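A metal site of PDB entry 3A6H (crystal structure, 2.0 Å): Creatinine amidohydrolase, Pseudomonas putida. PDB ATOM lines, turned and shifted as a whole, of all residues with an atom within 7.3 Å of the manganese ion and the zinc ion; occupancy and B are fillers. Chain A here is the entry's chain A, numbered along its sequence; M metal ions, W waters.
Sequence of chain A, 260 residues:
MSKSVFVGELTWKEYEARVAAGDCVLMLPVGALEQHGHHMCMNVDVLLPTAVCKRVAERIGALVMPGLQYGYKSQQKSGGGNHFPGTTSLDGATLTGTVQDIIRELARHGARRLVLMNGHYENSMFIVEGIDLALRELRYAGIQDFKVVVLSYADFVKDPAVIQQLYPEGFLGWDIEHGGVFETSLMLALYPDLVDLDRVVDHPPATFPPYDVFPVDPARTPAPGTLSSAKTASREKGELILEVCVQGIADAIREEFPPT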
ATOM      1  N   GLY A  31      26.963  -9.482 -13.706  1.00  0.00           N
ATOM      2  CA  GLY A  31      25.733  -8.734 -13.912  1.00  0.00           C
ATOM      3  C   GLY A  31      24.589  -9.448 -14.598  1.00  0.00           C
ATOM      4  O   GLY A  31      24.294 -10.606 -14.316  1.00  0.00           O
ATOM      5  N   ALA A  32      23.941  -8.730 -15.516  1.00  0.00           N
ATOM      6  CA  ALA A  32      22.804  -9.255 -16.239  1.00  0.00           C
ATOM      7  C   ALA A  32      22.308  -8.263 -17.288  1.00  0.00           C
ATOM      8  O   ALA A  32      22.680  -7.090 -17.262  1.00  0.00           O
ATOM      9  CB  ALA A  32      21.670  -9.549 -15.266  1.00  0.00           C
ATOM     10  N   GLU A  34      18.944  -6.936 -18.183  1.00  0.00           N
ATOM     11  CA  GLU A  34      17.612  -6.948 -17.592  1.00  0.00           C
ATOM     12  C   GLU A  34      16.926  -5.596 -17.673  1.00  0.00           C
ATOM     13  O   GLU A  34      17.554  -4.549 -17.490  1.00  0.00           O
ATOM     14  CB  GLU A  34      17.758  -7.360 -16.133  1.00  0.00           C
ATOM     15  CG  GLU A  34      16.486  -7.549 -15.330  1.00  0.00           C
ATOM     16  CD  GLU A  34      16.810  -7.709 -13.851  1.00  0.00           C
ATOM     17  OE1 GLU A  34      16.129  -8.484 -13.138  1.00  0.00           O
ATOM     18  OE2 GLU A  34      17.772  -7.037 -13.401  1.00  0.00           O
ATOM     19  N   GLN A  35      15.613  -5.617 -17.912  1.00  0.00           N
ATOM     20  CA  GLN A  35      14.842  -4.391 -18.000  1.00  0.00           C
ATOM     21  C   GLN A  35      14.975  -3.597 -16.713  1.00  0.00           C
ATOM     22  O   GLN A  35      14.946  -4.160 -15.610  1.00  0.00           O
ATOM     23  CB  GLN A  35      13.368  -4.695 -18.282  1.00  0.00           C
ATOM     24  CG  GLN A  35      12.581  -5.380 -17.155  1.00  0.00           C
ATOM     25  CD  GLN A  35      12.194  -4.433 -16.024  1.00  0.00           C
ATOM     26  OE1 GLN A  35      12.066  -3.224 -16.219  1.00  0.00           O
ATOM     27  NE2 GLN A  35      11.975  -4.992 -14.833  1.00  0.00           N
ATOM     28  N   HIS A  36      15.154  -2.287 -16.848  1.00  0.00           N
ATOM     29  CA  HIS A  36      15.260  -1.398 -15.701  1.00  0.00           C
ATOM     30  C   HIS A  36      14.325  -0.191 -15.880  1.00  0.00           C
ATOM     31  O   HIS A  36      14.750   0.952 -15.774  1.00  0.00           O
ATOM     32  CB  HIS A  36      16.689  -0.914 -15.494  1.00  0.00           C
ATOM     33  CG  HIS A  36      17.545  -1.881 -14.739  1.00  0.00           C
ATOM     34  ND1 HIS A  36      18.021  -3.056 -15.293  1.00  0.00           N
ATOM     35  CD2 HIS A  36      17.966  -1.883 -13.448  1.00  0.00           C
ATOM     36  CE1 HIS A  36      18.704  -3.724 -14.374  1.00  0.00           C
ATOM     37  NE2 HIS A  36      18.681  -3.031 -13.248  1.00  0.00           N
ATOM     38  N   MET A  40      15.951   3.780 -17.828  1.00  0.00           N
ATOM     39  CA  MET A  40      17.348   3.347 -17.868  1.00  0.00           C
ATOM     40  C   MET A  40      17.594   2.225 -18.866  1.00  0.00           C
ATOM     41  O   MET A  40      16.678   1.480 -19.222  1.00  0.00           O
ATOM     42  CB  MET A  40      17.814   2.882 -16.481  1.00  0.00           C
ATOM     43  CG  MET A  40      17.829   3.932 -15.416  1.00  0.00           C
ATOM     44  SD  MET A  40      18.888   3.441 -14.048  1.00  0.00           S
ATOM     45  CE  MET A  40      17.817   2.363 -13.107  1.00  0.00           C
ATOM     46  N   VAL A  44      22.464  -2.041 -16.835  1.00  0.00           N
ATOM     47  CA  VAL A  44      22.768  -1.456 -15.524  1.00  0.00           C
ATOM     48  C   VAL A  44      23.495  -2.417 -14.558  1.00  0.00           C
ATOM     49  O   VAL A  44      24.487  -2.037 -13.932  1.00  0.00           O
ATOM     50  CB  VAL A  44      21.473  -0.946 -14.841  1.00  0.00           C
ATOM     51  CG1 VAL A  44      21.730  -0.586 -13.375  1.00  0.00           C
ATOM     52  CG2 VAL A  44      20.926   0.276 -15.598  1.00  0.00           C
ATOM     53  N   ASP A  45      23.003  -3.648 -14.438  1.00  0.00           N
ATOM     54  CA  ASP A  45      23.621  -4.633 -13.540  1.00  0.00           C
ATOM     55  C   ASP A  45      25.063  -5.005 -13.906  1.00  0.00           C
ATOM     56  O   ASP A  45      25.765  -5.597 -13.094  1.00  0.00           O
ATOM     57  CB  ASP A  45      22.771  -5.897 -13.462  1.00  0.00           C
ATOM     58  CG  ASP A  45      21.474  -5.673 -12.710  1.00  0.00           C
ATOM     59  OD1 ASP A  45      21.311  -4.594 -12.108  1.00  0.00           O
ATOM     60  OD2 ASP A  45      20.614  -6.575 -12.712  1.00  0.00           O
ATOM     61  N   VAL A  46      25.486  -4.674 -15.119  1.00  0.00           N
ATOM     62  CA  VAL A  46      26.860  -4.942 -15.528  1.00  0.00           C
ATOM     63  C   VAL A  46      27.674  -3.667 -15.327  1.00  0.00           C
ATOM     64  O   VAL A  46      28.778  -3.696 -14.781  1.00  0.00           O
ATOM     65  CB  VAL A  46      26.979  -5.334 -17.028  1.00  0.00           C
ATOM     66  CG1 VAL A  46      28.453  -5.370 -17.433  1.00  0.00           C
ATOM     67  CG2 VAL A  46      26.348  -6.693 -17.278  1.00  0.00           C
ATOM     68  N   LEU A  48      27.184  -0.932 -13.338  1.00  0.00           N
ATOM     69  CA  LEU A  48      27.437  -0.514 -11.966  1.00  0.00           C
ATOM     70  C   LEU A  48      28.517  -1.281 -11.212  1.00  0.00           C
ATOM     71  O   LEU A  48      29.442  -0.679 -10.682  1.00  0.00           O
ATOM     72  CB  LEU A  48      26.124  -0.478 -11.181  1.00  0.00           C
ATOM     73  CG  LEU A  48      25.113   0.518 -11.772  1.00  0.00           C
ATOM     74  CD1 LEU A  48      23.920   0.650 -10.827  1.00  0.00           C
ATOM     75  CD2 LEU A  48      25.773   1.894 -11.984  1.00  0.00           C
ATOM     76  N   TYR A  72      21.209 -14.758 -13.957  1.00  0.00           N
ATOM     77  CA  TYR A  72      20.082 -15.643 -13.727  1.00  0.00           C
ATOM     78  C   TYR A  72      18.719 -14.967 -13.955  1.00  0.00           C
ATOM     79  O   TYR A  72      18.604 -13.747 -13.899  1.00  0.00           O
ATOM     80  CB  TYR A  72      20.127 -16.226 -12.307  1.00  0.00           C
ATOM     81  CG  TYR A  72      19.062 -17.284 -12.052  1.00  0.00           C
ATOM     82  CD1 TYR A  72      19.065 -18.490 -12.759  1.00  0.00           C
ATOM     83  CD2 TYR A  72      18.005 -17.038 -11.175  1.00  0.00           C
ATOM     84  CE1 TYR A  72      18.041 -19.426 -12.607  1.00  0.00           C
ATOM     85  CE2 TYR A  72      16.972 -17.966 -11.005  1.00  0.00           C
ATOM     86  CZ  TYR A  72      16.990 -19.153 -11.729  1.00  0.00           C
ATOM     87  OH  TYR A  72      15.952 -20.056 -11.603  1.00  0.00           O
ATOM     88  N   SER A  74      15.369 -13.177 -13.991  1.00  0.00           N
ATOM     89  CA  SER A  74      14.828 -12.091 -13.194  1.00  0.00           C
ATOM     90  C   SER A  74      13.635 -12.643 -12.395  1.00  0.00           C
ATOM     91  O   SER A  74      12.818 -13.389 -12.947  1.00  0.00           O
ATOM     92  CB  SER A  74      14.360 -10.960 -14.130  1.00  0.00           C
ATOM     93  OG  SER A  74      13.743  -9.910 -13.423  1.00  0.00           O
ATOM     94  N   SER A  78      12.033  -9.045  -7.004  1.00  0.00           N
ATOM     95  CA  SER A  78      13.348  -8.428  -6.931  1.00  0.00           C
ATOM     96  C   SER A  78      13.720  -7.677  -8.209  1.00  0.00           C
ATOM     97  O   SER A  78      14.296  -6.591  -8.146  1.00  0.00           O
ATOM     98  CB  SER A  78      14.427  -9.478  -6.608  1.00  0.00           C
ATOM     99  OG  SER A  78      14.404 -10.542  -7.539  1.00  0.00           O
ATOM    100  N   GLY A  79      13.381  -8.236  -9.363  1.00  0.00           N
ATOM    101  CA  GLY A  79      13.717  -7.596 -10.624  1.00  0.00           C
ATOM    102  C   GLY A  79      12.546  -7.390 -11.579  1.00  0.00           C
ATOM    103  O   GLY A  79      12.737  -6.981 -12.722  1.00  0.00           O
ATOM    104  N   GLY A 119      25.966  -7.733  -9.136  1.00  0.00           N
ATOM    105  CA  GLY A 119      25.174  -6.532  -9.341  1.00  0.00           C
ATOM    106  C   GLY A 119      23.733  -6.860  -9.691  1.00  0.00           C
ATOM    107  O   GLY A 119      22.941  -5.959  -9.962  1.00  0.00           O
ATOM    108  N   HIS A 120      23.398  -8.153  -9.667  1.00  0.00           N
ATOM    109  CA  HIS A 120      22.060  -8.663  -9.985  1.00  0.00           C
ATOM    110  C   HIS A 120      21.680  -9.667  -8.885  1.00  0.00           C
ATOM    111  O   HIS A 120      22.150 -10.819  -8.876  1.00  0.00           O
ATOM    112  CB  HIS A 120      22.109  -9.351 -11.363  1.00  0.00           C
ATOM    113  CG  HIS A 120      20.825 -10.018 -11.781  1.00  0.00           C
ATOM    114  ND1 HIS A 120      19.643  -9.334 -11.933  1.00  0.00           N
ATOM    115  CD2 HIS A 120      20.568 -11.293 -12.159  1.00  0.00           C
ATOM    116  CE1 HIS A 120      18.711 -10.157 -12.375  1.00  0.00           C
ATOM    117  NE2 HIS A 120      19.250 -11.349 -12.528  1.00  0.00           N
ATOM    118  N   TYR A 121      20.819  -9.240  -7.966  1.00  0.00           N
ATOM    119  CA  TYR A 121      20.382 -10.047  -6.826  1.00  0.00           C
ATOM    120  C   TYR A 121      20.163 -11.540  -7.092  1.00  0.00           C
ATOM    121  O   TYR A 121      20.691 -12.388  -6.371  1.00  0.00           O
ATOM    122  CB  TYR A 121      19.109  -9.443  -6.224  1.00  0.00           C
ATOM    123  CG  TYR A 121      18.706 -10.101  -4.935  1.00  0.00           C
ATOM    124  CD1 TYR A 121      19.512  -9.990  -3.801  1.00  0.00           C
ATOM    125  CD2 TYR A 121      17.544 -10.868  -4.844  1.00  0.00           C
ATOM    126  CE1 TYR A 121      19.173 -10.618  -2.615  1.00  0.00           C
ATOM    127  CE2 TYR A 121      17.193 -11.501  -3.657  1.00  0.00           C
ATOM    128  CZ  TYR A 121      18.015 -11.377  -2.546  1.00  0.00           C
ATOM    129  OH  TYR A 121      17.690 -12.001  -1.361  1.00  0.00           O
ATOM    130  N   GLU A 122      19.393 -11.846  -8.124  1.00  0.00           N
ATOM    131  CA  GLU A 122      19.087 -13.236  -8.484  1.00  0.00           C
ATOM    132  C   GLU A 122      20.294 -14.144  -8.744  1.00  0.00           C
ATOM    133  O   GLU A 122      20.156 -15.371  -8.687  1.00  0.00           O
ATOM    134  CB  GLU A 122      18.155 -13.257  -9.709  1.00  0.00           C
ATOM    135  CG  GLU A 122      16.752 -12.692  -9.436  1.00  0.00           C
ATOM    136  CD  GLU A 122      16.667 -11.184  -9.580  1.00  0.00           C
ATOM    137  OE1 GLU A 122      17.654 -10.479  -9.264  1.00  0.00           O
ATOM    138  OE2 GLU A 122      15.596 -10.701  -9.993  1.00  0.00           O
ATOM    139  N   ASN A 123      21.454 -13.561  -9.014  1.00  0.00           N
ATOM    140  CA  ASN A 123      22.671 -14.348  -9.282  1.00  0.00           C
ATOM    141  C   ASN A 123      23.260 -15.030  -8.058  1.00  0.00           C
ATOM    142  O   ASN A 123      23.882 -16.082  -8.173  1.00  0.00           O
ATOM    143  CB  ASN A 123      23.790 -13.470  -9.854  1.00  0.00           C
ATOM    144  CG  ASN A 123      23.524 -12.979 -11.254  1.00  0.00           C
ATOM    145  OD1 ASN A 123      22.837 -13.628 -12.038  1.00  0.00           O
ATOM    146  ND2 ASN A 123      24.095 -11.831 -11.593  1.00  0.00           N
ATOM    147  N   TYR A 153      27.652  -4.807  -3.934  1.00  0.00           N
ATOM    148  CA  TYR A 153      28.072  -3.462  -3.566  1.00  0.00           C
ATOM    149  C   TYR A 153      27.065  -2.651  -2.747  1.00  0.00           C
ATOM    150  O   TYR A 153      27.456  -1.883  -1.865  1.00  0.00           O
ATOM    151  CB  TYR A 153      28.506  -2.690  -4.820  1.00  0.00           C
ATOM    152  CG  TYR A 153      27.386  -2.308  -5.771  1.00  0.00           C
ATOM    153  CD1 TYR A 153      26.635  -1.164  -5.554  1.00  0.00           C
ATOM    154  CD2 TYR A 153      27.076  -3.114  -6.873  1.00  0.00           C
ATOM    155  CE1 TYR A 153      25.600  -0.811  -6.418  1.00  0.00           C
ATOM    156  CE2 TYR A 153      26.035  -2.768  -7.731  1.00  0.00           C
ATOM    157  CZ  TYR A 153      25.304  -1.614  -7.504  1.00  0.00           C
ATOM    158  OH  TYR A 153      24.259  -1.269  -8.332  1.00  0.00           O
ATOM    159  N   GLU A 177      13.879  -1.681  -4.445  1.00  0.00           N
ATOM    160  CA  GLU A 177      14.798  -0.817  -5.168  1.00  0.00           C
ATOM    161  C   GLU A 177      15.050  -1.026  -6.660  1.00  0.00           C
ATOM    162  O   GLU A 177      15.650  -0.154  -7.293  1.00  0.00           O
ATOM    163  CB  GLU A 177      16.140  -0.754  -4.422  1.00  0.00           C
ATOM    164  CG  GLU A 177      16.163   0.299  -3.329  1.00  0.00           C
ATOM    165  CD  GLU A 177      16.018   1.708  -3.866  1.00  0.00           C
ATOM    166  OE1 GLU A 177      15.508   2.582  -3.132  1.00  0.00           O
ATOM    167  OE2 GLU A 177      16.418   1.961  -5.032  1.00  0.00           O
ATOM    168  N   HIS A 178      14.609  -2.136  -7.245  1.00  0.00           N
ATOM    169  CA  HIS A 178      14.870  -2.358  -8.675  1.00  0.00           C
ATOM    170  C   HIS A 178      14.451  -1.162  -9.546  1.00  0.00           C
ATOM    171  O   HIS A 178      13.258  -0.853  -9.670  1.00  0.00           O
ATOM    172  CB  HIS A 178      14.156  -3.613  -9.169  1.00  0.00           C
ATOM    173  CG  HIS A 178      14.414  -3.921 -10.612  1.00  0.00           C
ATOM    174  ND1 HIS A 178      15.665  -4.216 -11.104  1.00  0.00           N
ATOM    175  CD2 HIS A 178      13.580  -3.957 -11.685  1.00  0.00           C
ATOM    176  CE1 HIS A 178      15.599  -4.424 -12.408  1.00  0.00           C
ATOM    177  NE2 HIS A 178      14.345  -4.275 -12.783  1.00  0.00           N
ATOM    178  N   GLY A 179      15.445  -0.515 -10.161  1.00  0.00           N
ATOM    179  CA  GLY A 179      15.192   0.639 -11.012  1.00  0.00           C
ATOM    180  C   GLY A 179      14.721   1.848 -10.223  1.00  0.00           C
ATOM    181  O   GLY A 179      14.174   2.805 -10.782  1.00  0.00           O
ATOM    182  N   GLU A 183      19.908   2.620  -7.698  1.00  0.00           N
ATOM    183  CA  GLU A 183      20.626   2.387  -8.947  1.00  0.00           C
ATOM    184  C   GLU A 183      20.545   3.569  -9.882  1.00  0.00           C
ATOM    185  O   GLU A 183      21.508   3.873 -10.586  1.00  0.00           O
ATOM    186  CB  GLU A 183      20.064   1.183  -9.708  1.00  0.00           C
ATOM    187  CG  GLU A 183      19.924  -0.088  -8.939  1.00  0.00           C
ATOM    188  CD  GLU A 183      19.423  -1.195  -9.832  1.00  0.00           C
ATOM    189  OE1 GLU A 183      20.261  -1.954 -10.351  1.00  0.00           O
ATOM    190  OE2 GLU A 183      18.192  -1.277 -10.055  1.00  0.00           O
HETATM  191 MN    MN M   1      18.944  -7.207 -11.412  1.00  0.00          MN
HETATM  192 ZN    ZN M   2      19.426  -3.728 -11.267  1.00  0.00          ZN
HETATM  193  O   HOH W   1      17.092  -7.946 -10.458  1.00  0.00           O
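Water W1 lies within hydrogen-bond range of OE1 of Glu 122 (2.9 Å) and OE1 of Glu 34 (2.9 Å).
Within 4 Å of the manganese ion: Glu 34, Asp 45 and His 120.
The zinc ion is bound by the side-chain carboxylate of Glu 183, a ring nitrogen (NE2) of His 36 and the side-chain carboxylate of Asp 45.
Residues that only touch the zinc ion: His 178 (3.8 Å). Within 4 Å of the zinc ion: His 36, Asp 45, His 178 and Glu 183. The nearest printed residue that does not touch the zinc ion is Glu 34 (4.3 Å).
The side-chain carboxylate of Glu 183 sits at hydrogen-bond distance from the backbone NH of Gly 179 (2.9 Å). ND1 of His 36 is in hydrogen-bond range of O of Glu 34. The backbone carbonyl oxygen (O) of His 120 sits close to the side-chain amide nitrogen (ND2) of Asn 123, at 3.5 Å. O of Tyr 72 sits at hydrogen-bond distance from NE2 of His 120 (2.8 Å). OE1 of Glu 34 sits at hydrogen-bond distance from OG of Ser 74 (2.8 Å). The backbone carbonyl oxygen (O) of Gly 79 lies within hydrogen-bond range of a ring nitrogen (NE2) of His 178 (3.1 Å). NE2 of His 178 is in hydrogen-bond range of O of Gln 35, at 2.9 Å.
The manganese ion is bound by the side-chain carboxylate of Asp 45 (2.2 Å), water W1 (2.2 Å), a ring nitrogen (ND1) of His 120 (2.3 Å) and the side-chain carboxylate of Glu 34 (2.3 Å).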
